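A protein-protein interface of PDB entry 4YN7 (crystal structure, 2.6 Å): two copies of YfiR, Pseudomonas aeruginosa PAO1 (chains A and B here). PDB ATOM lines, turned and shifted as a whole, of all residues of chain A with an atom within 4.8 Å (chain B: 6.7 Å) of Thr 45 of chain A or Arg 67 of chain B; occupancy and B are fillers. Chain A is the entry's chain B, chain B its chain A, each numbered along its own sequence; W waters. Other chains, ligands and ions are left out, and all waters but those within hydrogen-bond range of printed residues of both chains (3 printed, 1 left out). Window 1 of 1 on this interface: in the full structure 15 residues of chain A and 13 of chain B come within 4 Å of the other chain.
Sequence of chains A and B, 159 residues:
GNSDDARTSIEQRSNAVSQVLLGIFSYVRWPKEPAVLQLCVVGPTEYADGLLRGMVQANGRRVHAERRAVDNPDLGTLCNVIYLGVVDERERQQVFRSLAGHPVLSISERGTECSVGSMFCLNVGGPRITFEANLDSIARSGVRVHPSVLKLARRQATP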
ATOM      1  N   THR A   8     -23.039  13.806  -9.611  1.00  0.00           N
ATOM      2  CA  THR A   8     -24.440  13.718  -9.188  1.00  0.00           C
ATOM      3  C   THR A   8     -24.546  14.265  -7.767  1.00  0.00           C
ATOM      4  O   THR A   8     -23.538  14.447  -7.088  1.00  0.00           O
ATOM      5  CB  THR A   8     -25.014  12.269  -9.295  1.00  0.00           C
ATOM      6  OG1 THR A   8     -24.444  11.401  -8.297  1.00  0.00           O
ATOM      7  CG2 THR A   8     -24.737  11.674 -10.694  1.00  0.00           C
ATOM      8  N   ILE A  10     -25.712  12.596  -5.383  1.00  0.00           N
ATOM      9  CA  ILE A  10     -25.336  11.472  -4.532  1.00  0.00           C
ATOM     10  C   ILE A  10     -23.836  11.460  -4.349  1.00  0.00           C
ATOM     11  O   ILE A  10     -23.354  11.277  -3.243  1.00  0.00           O
ATOM     12  CB  ILE A  10     -25.837  10.116  -5.082  1.00  0.00           C
ATOM     13  CG1 ILE A  10     -27.361  10.125  -5.240  1.00  0.00           C
ATOM     14  CG2 ILE A  10     -25.466   8.984  -4.135  1.00  0.00           C
ATOM     15  CD1 ILE A  10     -28.122  10.268  -3.936  1.00  0.00           C
ATOM     16  N   GLU A  11     -23.102  11.682  -5.427  1.00  0.00           N
ATOM     17  CA  GLU A  11     -21.643  11.765  -5.347  1.00  0.00           C
ATOM     18  C   GLU A  11     -21.137  12.957  -4.528  1.00  0.00           C
ATOM     19  O   GLU A  11     -20.194  12.822  -3.749  1.00  0.00           O
ATOM     20  CB  GLU A  11     -21.035  11.800  -6.734  1.00  0.00           C
ATOM     21  CG  GLU A  11     -21.045  10.437  -7.395  1.00  0.00           C
ATOM     22  CD  GLU A  11     -21.055  10.502  -8.917  1.00  0.00           C
ATOM     23  OE1 GLU A  11     -21.315   9.447  -9.541  1.00  0.00           O
ATOM     24  OE2 GLU A  11     -20.800  11.592  -9.495  1.00  0.00           O
ATOM     25  N   VAL A  41     -18.374  -0.732   6.739  1.00  0.00           N
ATOM     26  CA  VAL A  41     -19.644  -0.336   6.235  1.00  0.00           C
ATOM     27  C   VAL A  41     -20.569  -1.540   6.235  1.00  0.00           C
ATOM     28  O   VAL A  41     -20.316  -2.495   5.615  1.00  0.00           O
ATOM     29  CB  VAL A  41     -19.488   0.232   4.830  1.00  0.00           C
ATOM     30  CG1 VAL A  41     -20.801   0.664   4.264  1.00  0.00           C
ATOM     31  CG2 VAL A  41     -18.561   1.405   4.865  1.00  0.00           C
ATOM     32  N   GLY A  43     -24.540  -2.936   5.935  1.00  0.00           N
ATOM     33  CA  GLY A  43     -25.897  -2.732   5.485  1.00  0.00           C
ATOM     34  C   GLY A  43     -25.986  -1.919   4.197  1.00  0.00           C
ATOM     35  O   GLY A  43     -25.021  -1.343   3.751  1.00  0.00           O
ATOM     36  N   PRO A  44     -27.170  -1.858   3.601  1.00  0.00           N
ATOM     37  CA  PRO A  44     -27.396  -1.025   2.447  1.00  0.00           C
ATOM     38  C   PRO A  44     -27.116   0.442   2.739  1.00  0.00           C
ATOM     39  O   PRO A  44     -27.610   0.968   3.724  1.00  0.00           O
ATOM     40  CB  PRO A  44     -28.879  -1.210   2.164  1.00  0.00           C
ATOM     41  CG  PRO A  44     -29.219  -2.508   2.785  1.00  0.00           C
ATOM     42  CD  PRO A  44     -28.352  -2.635   3.976  1.00  0.00           C
ATOM     43  N   THR A  45     -26.346   1.096   1.870  1.00  0.00           N
ATOM     44  CA  THR A  45     -26.022   2.513   2.018  1.00  0.00           C
ATOM     45  C   THR A  45     -26.062   3.219   0.674  1.00  0.00           C
ATOM     46  O   THR A  45     -25.784   2.600  -0.354  1.00  0.00           O
ATOM     47  CB  THR A  45     -24.625   2.691   2.606  1.00  0.00           C
ATOM     48  OG1 THR A  45     -23.643   2.091   1.740  1.00  0.00           O
ATOM     49  CG2 THR A  45     -24.542   2.062   3.990  1.00  0.00           C
ATOM     50  N   GLU A  46     -26.438   4.502   0.690  1.00  0.00           N
ATOM     51  CA  GLU A  46     -26.359   5.395  -0.470  1.00  0.00           C
ATOM     52  C   GLU A  46     -25.077   6.204  -0.535  1.00  0.00           C
ATOM     53  O   GLU A  46     -24.635   6.590  -1.635  1.00  0.00           O
ATOM     54  CB  GLU A  46     -27.473   6.414  -0.450  1.00  0.00           C
ATOM     55  CG  GLU A  46     -28.803   5.923  -0.974  1.00  0.00           C
ATOM     56  CD  GLU A  46     -29.845   7.017  -1.041  1.00  0.00           C
ATOM     57  OE1 GLU A  46     -30.112   7.501  -2.165  1.00  0.00           O
ATOM     58  OE2 GLU A  46     -30.392   7.365   0.026  1.00  0.00           O
ATOM     59  N   TYR A  47     -24.484   6.498   0.615  1.00  0.00           N
ATOM     60  CA  TYR A  47     -23.475   7.568   0.644  1.00  0.00           C
ATOM     61  C   TYR A  47     -22.098   7.154   1.104  1.00  0.00           C
ATOM     62  O   TYR A  47     -21.301   7.999   1.512  1.00  0.00           O
ATOM     63  CB  TYR A  47     -23.977   8.736   1.508  1.00  0.00           C
ATOM     64  CG  TYR A  47     -25.302   9.320   1.060  1.00  0.00           C
ATOM     65  CD1 TYR A  47     -25.391  10.093  -0.085  1.00  0.00           C
ATOM     66  CD2 TYR A  47     -26.449   9.110   1.792  1.00  0.00           C
ATOM     67  CE1 TYR A  47     -26.597  10.629  -0.496  1.00  0.00           C
ATOM     68  CE2 TYR A  47     -27.656   9.653   1.400  1.00  0.00           C
ATOM     69  CZ  TYR A  47     -27.727  10.405   0.251  1.00  0.00           C
ATOM     70  OH  TYR A  47     -28.937  10.929  -0.143  1.00  0.00           O
ATOM     71  N   ALA A  48     -21.812   5.859   1.042  1.00  0.00           N
ATOM     72  CA  ALA A  48     -20.548   5.347   1.554  1.00  0.00           C
ATOM     73  C   ALA A  48     -19.457   5.154   0.484  1.00  0.00           C
ATOM     74  O   ALA A  48     -18.353   4.734   0.803  1.00  0.00           O
ATOM     75  CB  ALA A  48     -20.791   4.066   2.339  1.00  0.00           C
ATOM     76  N   ASP A  49     -19.742   5.472  -0.776  1.00  0.00           N
ATOM     77  CA  ASP A  49     -18.740   5.254  -1.839  1.00  0.00           C
ATOM     78  C   ASP A  49     -17.470   6.045  -1.644  1.00  0.00           C
ATOM     79  O   ASP A  49     -16.410   5.598  -2.063  1.00  0.00           O
ATOM     80  CB  ASP A  49     -19.315   5.551  -3.215  1.00  0.00           C
ATOM     81  CG  ASP A  49     -20.280   4.482  -3.680  1.00  0.00           C
ATOM     82  OD1 ASP A  49     -20.311   3.403  -3.039  1.00  0.00           O
ATOM     83  OD2 ASP A  49     -21.003   4.717  -4.687  1.00  0.00           O
ATOM     84  N   ARG A  67     -16.672  -3.264   3.265  1.00  0.00           N
ATOM     85  CA  ARG A  67     -17.989  -3.753   3.560  1.00  0.00           C
ATOM     86  C   ARG A  67     -17.934  -5.042   4.296  1.00  0.00           C
ATOM     87  O   ARG A  67     -17.147  -5.889   3.989  1.00  0.00           O
ATOM     88  CB  ARG A  67     -18.769  -3.978   2.291  1.00  0.00           C
ATOM     89  CG  ARG A  67     -19.647  -2.821   1.989  1.00  0.00           C
ATOM     90  CD  ARG A  67     -20.454  -3.020   0.733  1.00  0.00           C
ATOM     91  NE  ARG A  67     -20.975  -1.723   0.333  1.00  0.00           N
ATOM     92  CZ  ARG A  67     -21.961  -1.140   0.962  1.00  0.00           C
ATOM     93  NH1 ARG A  67     -22.512  -1.744   1.975  1.00  0.00           N
ATOM     94  NH2 ARG A  67     -22.399   0.020   0.595  1.00  0.00           N
ATOM     95  N   TYR A  83     -19.958   2.078  10.048  1.00  0.00           N
ATOM     96  CA  TYR A  83     -20.877   2.973   9.383  1.00  0.00           C
ATOM     97  C   TYR A  83     -22.062   2.127   9.005  1.00  0.00           C
ATOM     98  O   TYR A  83     -21.956   1.233   8.182  1.00  0.00           O
ATOM     99  CB  TYR A  83     -20.207   3.590   8.147  1.00  0.00           C
ATOM    100  CG  TYR A  83     -21.076   4.570   7.386  1.00  0.00           C
ATOM    101  CD1 TYR A  83     -21.207   5.888   7.801  1.00  0.00           C
ATOM    102  CD2 TYR A  83     -21.764   4.173   6.254  1.00  0.00           C
ATOM    103  CE1 TYR A  83     -21.998   6.785   7.105  1.00  0.00           C
ATOM    104  CE2 TYR A  83     -22.554   5.056   5.551  1.00  0.00           C
ATOM    105  CZ  TYR A  83     -22.668   6.370   5.979  1.00  0.00           C
ATOM    106  OH  TYR A  83     -23.472   7.241   5.278  1.00  0.00           O
ATOM    107  N   LEU A  84     -23.201   2.404   9.612  1.00  0.00           N
ATOM    108  CA  LEU A  84     -24.328   1.502   9.546  1.00  0.00           C
ATOM    109  C   LEU A  84     -25.447   1.958   8.620  1.00  0.00           C
ATOM    110  O   LEU A  84     -25.979   3.061   8.750  1.00  0.00           O
ATOM    111  CB  LEU A  84     -24.870   1.288  10.953  1.00  0.00           C
ATOM    112  CG  LEU A  84     -25.927   0.205  11.137  1.00  0.00           C
ATOM    113  CD1 LEU A  84     -25.359  -1.153  10.750  1.00  0.00           C
ATOM    114  CD2 LEU A  84     -26.376   0.202  12.594  1.00  0.00           C
ATOM    115  N   GLY A  85     -25.814   1.076   7.697  1.00  0.00           N
ATOM    116  CA  GLY A  85     -26.853   1.352   6.746  1.00  0.00           C
ATOM    117  C   GLY A  85     -28.240   0.946   7.214  1.00  0.00           C
ATOM    118  O   GLY A  85     -28.494   0.796   8.392  1.00  0.00           O
ATOM    119  N   GLU A 109     -26.172   6.015   8.773  1.00  0.00           N
ATOM    120  CA  GLU A 109     -26.342   6.911   7.638  1.00  0.00           C
ATOM    121  C   GLU A 109     -27.660   7.662   7.705  1.00  0.00           C
ATOM    122  O   GLU A 109     -27.746   8.806   7.285  1.00  0.00           O
ATOM    123  CB  GLU A 109     -26.261   6.092   6.342  1.00  0.00           C
ATOM    124  CG  GLU A 109     -26.762   6.819   5.120  1.00  0.00           C
ATOM    125  CD  GLU A 109     -26.385   6.117   3.853  1.00  0.00           C
ATOM    126  OE1 GLU A 109     -25.190   6.128   3.513  1.00  0.00           O
ATOM    127  OE2 GLU A 109     -27.285   5.550   3.214  1.00  0.00           O
ATOM    128  N   LEU B  39     -26.126   2.775 -16.470  1.00  0.00           N
ATOM    129  CA  LEU B  39     -26.765   2.208 -15.330  1.00  0.00           C
ATOM    130  C   LEU B  39     -26.833   3.194 -14.217  1.00  0.00           C
ATOM    131  O   LEU B  39     -25.899   3.827 -13.907  1.00  0.00           O
ATOM    132  CB  LEU B  39     -26.048   0.975 -14.881  1.00  0.00           C
ATOM    133  CG  LEU B  39     -26.795  -0.011 -14.039  1.00  0.00           C
ATOM    134  CD1 LEU B  39     -26.244  -1.321 -14.433  1.00  0.00           C
ATOM    135  CD2 LEU B  39     -26.523   0.172 -12.582  1.00  0.00           C
ATOM    136  N   CYS B  40     -27.996   3.318 -13.633  1.00  0.00           N
ATOM    137  CA  CYS B  40     -28.157   4.089 -12.441  1.00  0.00           C
ATOM    138  C   CYS B  40     -28.466   3.250 -11.245  1.00  0.00           C
ATOM    139  O   CYS B  40     -29.370   2.511 -11.242  1.00  0.00           O
ATOM    140  CB  CYS B  40     -29.231   5.140 -12.617  1.00  0.00           C
ATOM    141  SG  CYS B  40     -28.881   6.211 -13.997  1.00  0.00           S
ATOM    142  N   VAL B  41     -27.706   3.440 -10.200  1.00  0.00           N
ATOM    143  CA  VAL B  41     -27.994   2.839  -8.924  1.00  0.00           C
ATOM    144  C   VAL B  41     -28.824   3.782  -8.055  1.00  0.00           C
ATOM    145  O   VAL B  41     -28.454   4.863  -7.813  1.00  0.00           O
ATOM    146  CB  VAL B  41     -26.697   2.351  -8.222  1.00  0.00           C
ATOM    147  CG1 VAL B  41     -26.991   1.766  -6.884  1.00  0.00           C
ATOM    148  CG2 VAL B  41     -26.040   1.311  -9.051  1.00  0.00           C
ATOM    149  N   VAL B  42     -29.988   3.339  -7.634  1.00  0.00           N
ATOM    150  CA  VAL B  42     -30.887   4.222  -6.914  1.00  0.00           C
ATOM    151  C   VAL B  42     -31.271   3.629  -5.556  1.00  0.00           C
ATOM    152  O   VAL B  42     -31.840   2.564  -5.490  1.00  0.00           O
ATOM    153  CB  VAL B  42     -32.137   4.514  -7.775  1.00  0.00           C
ATOM    154  CG1 VAL B  42     -33.219   5.235  -6.988  1.00  0.00           C
ATOM    155  CG2 VAL B  42     -31.756   5.347  -8.981  1.00  0.00           C
ATOM    156  N   GLY B  43     -30.974   4.344  -4.482  1.00  0.00           N
ATOM    157  CA  GLY B  43     -31.340   3.911  -3.132  1.00  0.00           C
ATOM    158  C   GLY B  43     -30.201   3.158  -2.471  1.00  0.00           C
ATOM    159  O   GLY B  43     -29.246   2.779  -3.119  1.00  0.00           O
ATOM    160  N   PRO B  44     -30.294   2.918  -1.173  1.00  0.00           N
ATOM    161  CA  PRO B  44     -29.204   2.249  -0.488  1.00  0.00           C
ATOM    162  C   PRO B  44     -28.991   0.821  -0.971  1.00  0.00           C
ATOM    163  O   PRO B  44     -29.958   0.077  -1.104  1.00  0.00           O
ATOM    164  CB  PRO B  44     -29.657   2.225   0.981  1.00  0.00           C
ATOM    165  CG  PRO B  44     -30.878   3.076   1.051  1.00  0.00           C
ATOM    166  CD  PRO B  44     -31.463   3.104  -0.312  1.00  0.00           C
ATOM    167  N   THR B  45     -27.736   0.440  -1.208  1.00  0.00           N
ATOM    168  CA  THR B  45     -27.417  -0.898  -1.681  1.00  0.00           C
ATOM    169  C   THR B  45     -26.247  -1.529  -0.915  1.00  0.00           C
ATOM    170  O   THR B  45     -25.375  -0.843  -0.403  1.00  0.00           O
ATOM    171  CB  THR B  45     -27.073  -0.898  -3.186  1.00  0.00           C
ATOM    172  OG1 THR B  45     -25.999  -0.011  -3.436  1.00  0.00           O
ATOM    173  CG2 THR B  45     -28.239  -0.466  -4.019  1.00  0.00           C
ATOM    174  N   GLU B  46     -26.247  -2.852  -0.839  1.00  0.00           N
ATOM    175  CA  GLU B  46     -25.139  -3.602  -0.240  1.00  0.00           C
ATOM    176  C   GLU B  46     -24.197  -4.177  -1.259  1.00  0.00           C
ATOM    177  O   GLU B  46     -23.030  -4.380  -0.949  1.00  0.00           O
ATOM    178  CB  GLU B  46     -25.656  -4.779   0.539  1.00  0.00           C
ATOM    179  CG  GLU B  46     -25.833  -4.482   1.980  1.00  0.00           C
ATOM    180  CD  GLU B  46     -26.191  -5.708   2.753  1.00  0.00           C
ATOM    181  OE1 GLU B  46     -25.277  -6.210   3.438  1.00  0.00           O
ATOM    182  OE2 GLU B  46     -27.376  -6.124   2.650  1.00  0.00           O
ATOM    183  N   ALA B  48     -23.789  -3.305  -4.775  1.00  0.00           N
ATOM    184  CA  ALA B  48     -23.561  -2.562  -6.010  1.00  0.00           C
ATOM    185  C   ALA B  48     -22.129  -2.033  -6.166  1.00  0.00           C
ATOM    186  O   ALA B  48     -21.804  -1.473  -7.197  1.00  0.00           O
ATOM    187  CB  ALA B  48     -24.540  -1.412  -6.110  1.00  0.00           C
ATOM    188  N   ASP B  49     -21.263  -2.226  -5.176  1.00  0.00           N
ATOM    189  CA  ASP B  49     -19.883  -1.683  -5.276  1.00  0.00           C
ATOM    190  C   ASP B  49     -19.132  -2.210  -6.504  1.00  0.00           C
ATOM    191  O   ASP B  49     -18.338  -1.489  -7.093  1.00  0.00           O
ATOM    192  CB  ASP B  49     -19.079  -1.938  -3.997  1.00  0.00           C
ATOM    193  CG  ASP B  49     -19.662  -1.210  -2.772  1.00  0.00           C
ATOM    194  OD1 ASP B  49     -20.590  -0.355  -2.919  1.00  0.00           O
ATOM    195  OD2 ASP B  49     -19.198  -1.510  -1.642  1.00  0.00           O
ATOM    196  N   LEU B  52     -20.575  -0.504  -9.755  1.00  0.00           N
ATOM    197  CA  LEU B  52     -20.220   0.899  -9.815  1.00  0.00           C
ATOM    198  C   LEU B  52     -18.821   1.165 -10.343  1.00  0.00           C
ATOM    199  O   LEU B  52     -18.503   2.297 -10.641  1.00  0.00           O
ATOM    200  CB  LEU B  52     -20.474   1.565  -8.465  1.00  0.00           C
ATOM    201  CG  LEU B  52     -21.962   1.854  -8.224  1.00  0.00           C
ATOM    202  CD1 LEU B  52     -22.275   1.985  -6.761  1.00  0.00           C
ATOM    203  CD2 LEU B  52     -22.423   3.111  -8.945  1.00  0.00           C
ATOM    204  N   ALA B  65     -21.787   3.180 -14.831  1.00  0.00           N
ATOM    205  CA  ALA B  65     -22.693   3.108 -13.692  1.00  0.00           C
ATOM    206  C   ALA B  65     -22.487   4.289 -12.752  1.00  0.00           C
ATOM    207  O   ALA B  65     -21.376   4.723 -12.525  1.00  0.00           O
ATOM    208  CB  ALA B  65     -22.458   1.812 -12.947  1.00  0.00           C
ATOM    209  N   GLU B  66     -23.572   4.798 -12.192  1.00  0.00           N
ATOM    210  CA  GLU B  66     -23.489   5.814 -11.148  1.00  0.00           C
ATOM    211  C   GLU B  66     -24.734   5.815 -10.272  1.00  0.00           C
ATOM    212  O   GLU B  66     -25.788   5.358 -10.702  1.00  0.00           O
ATOM    213  CB  GLU B  66     -23.315   7.179 -11.781  1.00  0.00           C
ATOM    214  CG  GLU B  66     -24.504   7.622 -12.612  1.00  0.00           C
ATOM    215  CD  GLU B  66     -24.178   8.799 -13.504  1.00  0.00           C
ATOM    216  OE1 GLU B  66     -23.042   9.329 -13.409  1.00  0.00           O
ATOM    217  OE2 GLU B  66     -25.076   9.197 -14.285  1.00  0.00           O
ATOM    218  N   ARG B  67     -24.607   6.352  -9.058  1.00  0.00           N
ATOM    219  CA  ARG B  67     -25.747   6.467  -8.150  1.00  0.00           C
ATOM    220  C   ARG B  67     -26.541   7.717  -8.457  1.00  0.00           C
ATOM    221  O   ARG B  67     -25.976   8.712  -8.833  1.00  0.00           O
ATOM    222  CB  ARG B  67     -25.340   6.499  -6.667  1.00  0.00           C
ATOM    223  CG  ARG B  67     -24.218   5.577  -6.275  1.00  0.00           C
ATOM    224  CD  ARG B  67     -24.030   5.528  -4.768  1.00  0.00           C
ATOM    225  NE  ARG B  67     -24.851   4.461  -4.252  1.00  0.00           N
ATOM    226  CZ  ARG B  67     -24.414   3.291  -3.835  1.00  0.00           C
ATOM    227  NH1 ARG B  67     -23.116   3.009  -3.804  1.00  0.00           N
ATOM    228  NH2 ARG B  67     -25.305   2.398  -3.431  1.00  0.00           N
ATOM    229  N   ARG B  68     -27.862   7.654  -8.289  1.00  0.00           N
ATOM    230  CA  ARG B  68     -28.730   8.823  -8.473  1.00  0.00           C
ATOM    231  C   ARG B  68     -29.795   8.878  -7.411  1.00  0.00           C
ATOM    232  O   ARG B  68     -30.120   7.868  -6.792  1.00  0.00           O
ATOM    233  CB  ARG B  68     -29.354   8.830  -9.854  1.00  0.00           C
ATOM    234  CG  ARG B  68     -28.338   9.175 -10.928  1.00  0.00           C
ATOM    235  CD  ARG B  68     -28.978   9.438 -12.268  1.00  0.00           C
ATOM    236  NE  ARG B  68     -27.974   9.872 -13.231  1.00  0.00           N
ATOM    237  CZ  ARG B  68     -27.456  11.099 -13.271  1.00  0.00           C
ATOM    238  NH1 ARG B  68     -27.847  12.039 -12.398  1.00  0.00           N
ATOM    239  NH2 ARG B  68     -26.545  11.389 -14.189  1.00  0.00           N
ATOM    240  N   ALA B  69     -30.309  10.076  -7.179  1.00  0.00           N
ATOM    241  CA  ALA B  69     -31.292  10.284  -6.131  1.00  0.00           C
ATOM    242  C   ALA B  69     -32.578   9.584  -6.486  1.00  0.00           C
ATOM    243  O   ALA B  69     -32.979   9.535  -7.638  1.00  0.00           O
ATOM    244  CB  ALA B  69     -31.559  11.762  -5.908  1.00  0.00           C
HETATM  245  O   HOH W   1     -29.385   6.677  -4.520  1.00  0.00           O
HETATM  246  O   HOH W   2     -22.953   3.437  -0.642  1.00  0.00           O
HETATM  247  O   HOH W   3     -22.956  -4.794   3.989  1.00  0.00           O
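O of Arg 67 of chain B lies within hydrogen-bond range of OG1 of Thr 8 of chain A (3.1 Å).
OD2 of Asp 49 of chain A lies within salt-bridge range of NH1 of Arg 67 of chain B, 2.9 Å away.
The backbone carbonyl oxygen (O) of Thr 45 of chain B lies within hydrogen-bond range of the guanidinium group (NH2) of Arg 67 of chain A, 3.3 Å away.
The backbone NH (N) of Thr 45 of chain B sits at hydrogen-bond distance from the backbone carbonyl oxygen (O) of Thr 45 of chain A.
NE of Arg 67 of chain B sits close to O of Glu 46 of chain A.
OD2 of Asp 49 of chain B is in salt-bridge range of NE of Arg 67 of chain A (2.7 Å).
The guanidinium group (NH2) of Arg 67 of chain B sits at hydrogen-bond distance from the backbone carbonyl oxygen (O) of Thr 45 of chain A (3.1 Å).
N of Thr 8 of chain A is in hydrogen-bond range of OE2 of Glu 11 of chain A, 3.2 Å away.
The backbone carbonyl oxygen (O) of Leu 39 of chain B is in hydrogen-bond range of the backbone NH (N) of Glu 66 of chain B, at 3.0 Å.
O of Val 41 of chain B lies within hydrogen-bond range of N of Arg 68 of chain B.
The guanidinium group (NH1) of Arg 67 of chain A lies within hydrogen-bond range of the backbone carbonyl oxygen (O) of Gly 43 of chain A (3.1 Å).
The side-chain carboxylate (OE2) of Glu 66 of chain B is in salt-bridge range of the guanidinium group (NH2) of Arg 68 of chain B.
The side-chain hydroxyl of Thr 45 of chain A sits at hydrogen-bond distance from the guanidinium group of Arg 67 of chain A.
Glu 66 of chain B touches Thr 8 of chain A.
Thr 8 of chain A touches Arg 68 of chain B (CG2 to NH1, 3.6 Å).
Ala 69 of chain B touches Ile 10 of chain A.
Glu 11 of chain A touches Glu 66 of chain B.
Pro 44 of chain A touches Pro 44 of chain B.
Thr 45 of chain B touches Pro 44 of chain A (O to CA, 3.5 Å).
Pro 44 of chain B touches Thr 45 of chain A.
Gly 43 of chain B touches Glu 46 of chain A.
Glu 46 of chain A touches Pro 44 of chain B (CG to N, 3.4 Å).
O of Glu 46 of chain B touches CD of Arg 67 of chain A, 3.4 Å away.
Of chain A, only Thr 8, Ile 10, Thr 45, Glu 46 and Asp 49 come within 4 Å of Arg 67 of chain B.
Of the printed residues of chain A, Glu 46 of chain B touches Gly 43 (3.4 Å), Pro 44 (3.4 Å) and Arg 67 (3.4 Å).
Of the printed residues of chain B, Asp 49 of chain A touches Asp 49 (3.8 Å), Leu 52 (3.7 Å) and Arg 67 (2.9 Å).
Ala 48 of chain A touches none of the printed residues of chain B.
The nearest residue of chain B that does not touch Thr 45 of chain A is Gly 43 of chain B (4.4 Å).
The nearest residue of chain A that does not touch Arg 67 of chain B is Glu 11 of chain A (4.5 Å).
The nearest printed residue of chain A that does not touch Ala 69 of chain B is Glu 46 of chain A (5.0 Å).
Of the 16 printed residues of chain A, 9 touch a printed residue of chain B.
Of the 16 printed residues of chain B, 10 touch a printed residue of chain A.
Printed residues of chain B that touch a printed residue of chain A: Gly 43, Pro 44, Thr 45, Glu 46, Asp 49, Leu 52, Glu 66, Arg 67, Arg 68 and Ala 69.
Hydrophobic or aromatic side chains of chain B within 4 Å of the printed part of chain A: Pro 44 and Leu 52.
Along chain B the printed residues that touch a printed residue of chain A span positions 43 to 69.
Among the printed residues, 23 pairs touch across the chains.
Among the printed residues, Asp or Glu carboxylates within 4 Å of a Lys or Arg side-chain nitrogen of the other chain: Asp 49 of chain A with Arg 67 of chain B (2.9 Å) and Arg 67 of chain A with Asp 49 of chain B (2.7 Å).
Pro 44 of chain A touches Glu 46 of chain B, and with the chains exchanged Glu 46 of chain A touches Pro 44 of chain B.
Thr 45 of chain B touches its own counterpart, Thr 45 of chain A.
Thr 45 of chain A touches Arg 67 of chain B, and with the chains exchanged Arg 67 of chain A touches Thr 45 of chain B.
Glu 46 of chain A touches Arg 67 of chain B, and with the chains exchanged Arg 67 of chain A touches Glu 46 of chain B.
Positions printed for both chains: 41, 43, 44, 45, 46, 48, 49 and 67.
Of the 23 pairs that touch across the chains among the printed residues, 15 have their exchanged pair printed and touching as well.
Water W1 lies within hydrogen-bond range of the side-chain carboxylate (OE1) of Glu 46 of chain A, the backbone carbonyl oxygen (O) of Arg 68 of chain B and the backbone NH (N) of Gly 43 of chain B.
Water W3 bridges OE1 of Glu 46 of chain B (2.8 Å) and N of Gly 43 of chain A (3.1 Å).
Water W2 lies within hydrogen-bond range of the side-chain hydroxyl of Thr 45 of chain A (2.8 Å), the backbone NH of Ala 48 of chain A (3.2 Å) and the guanidinium group of Arg 67 of chain B (3.2 Å).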
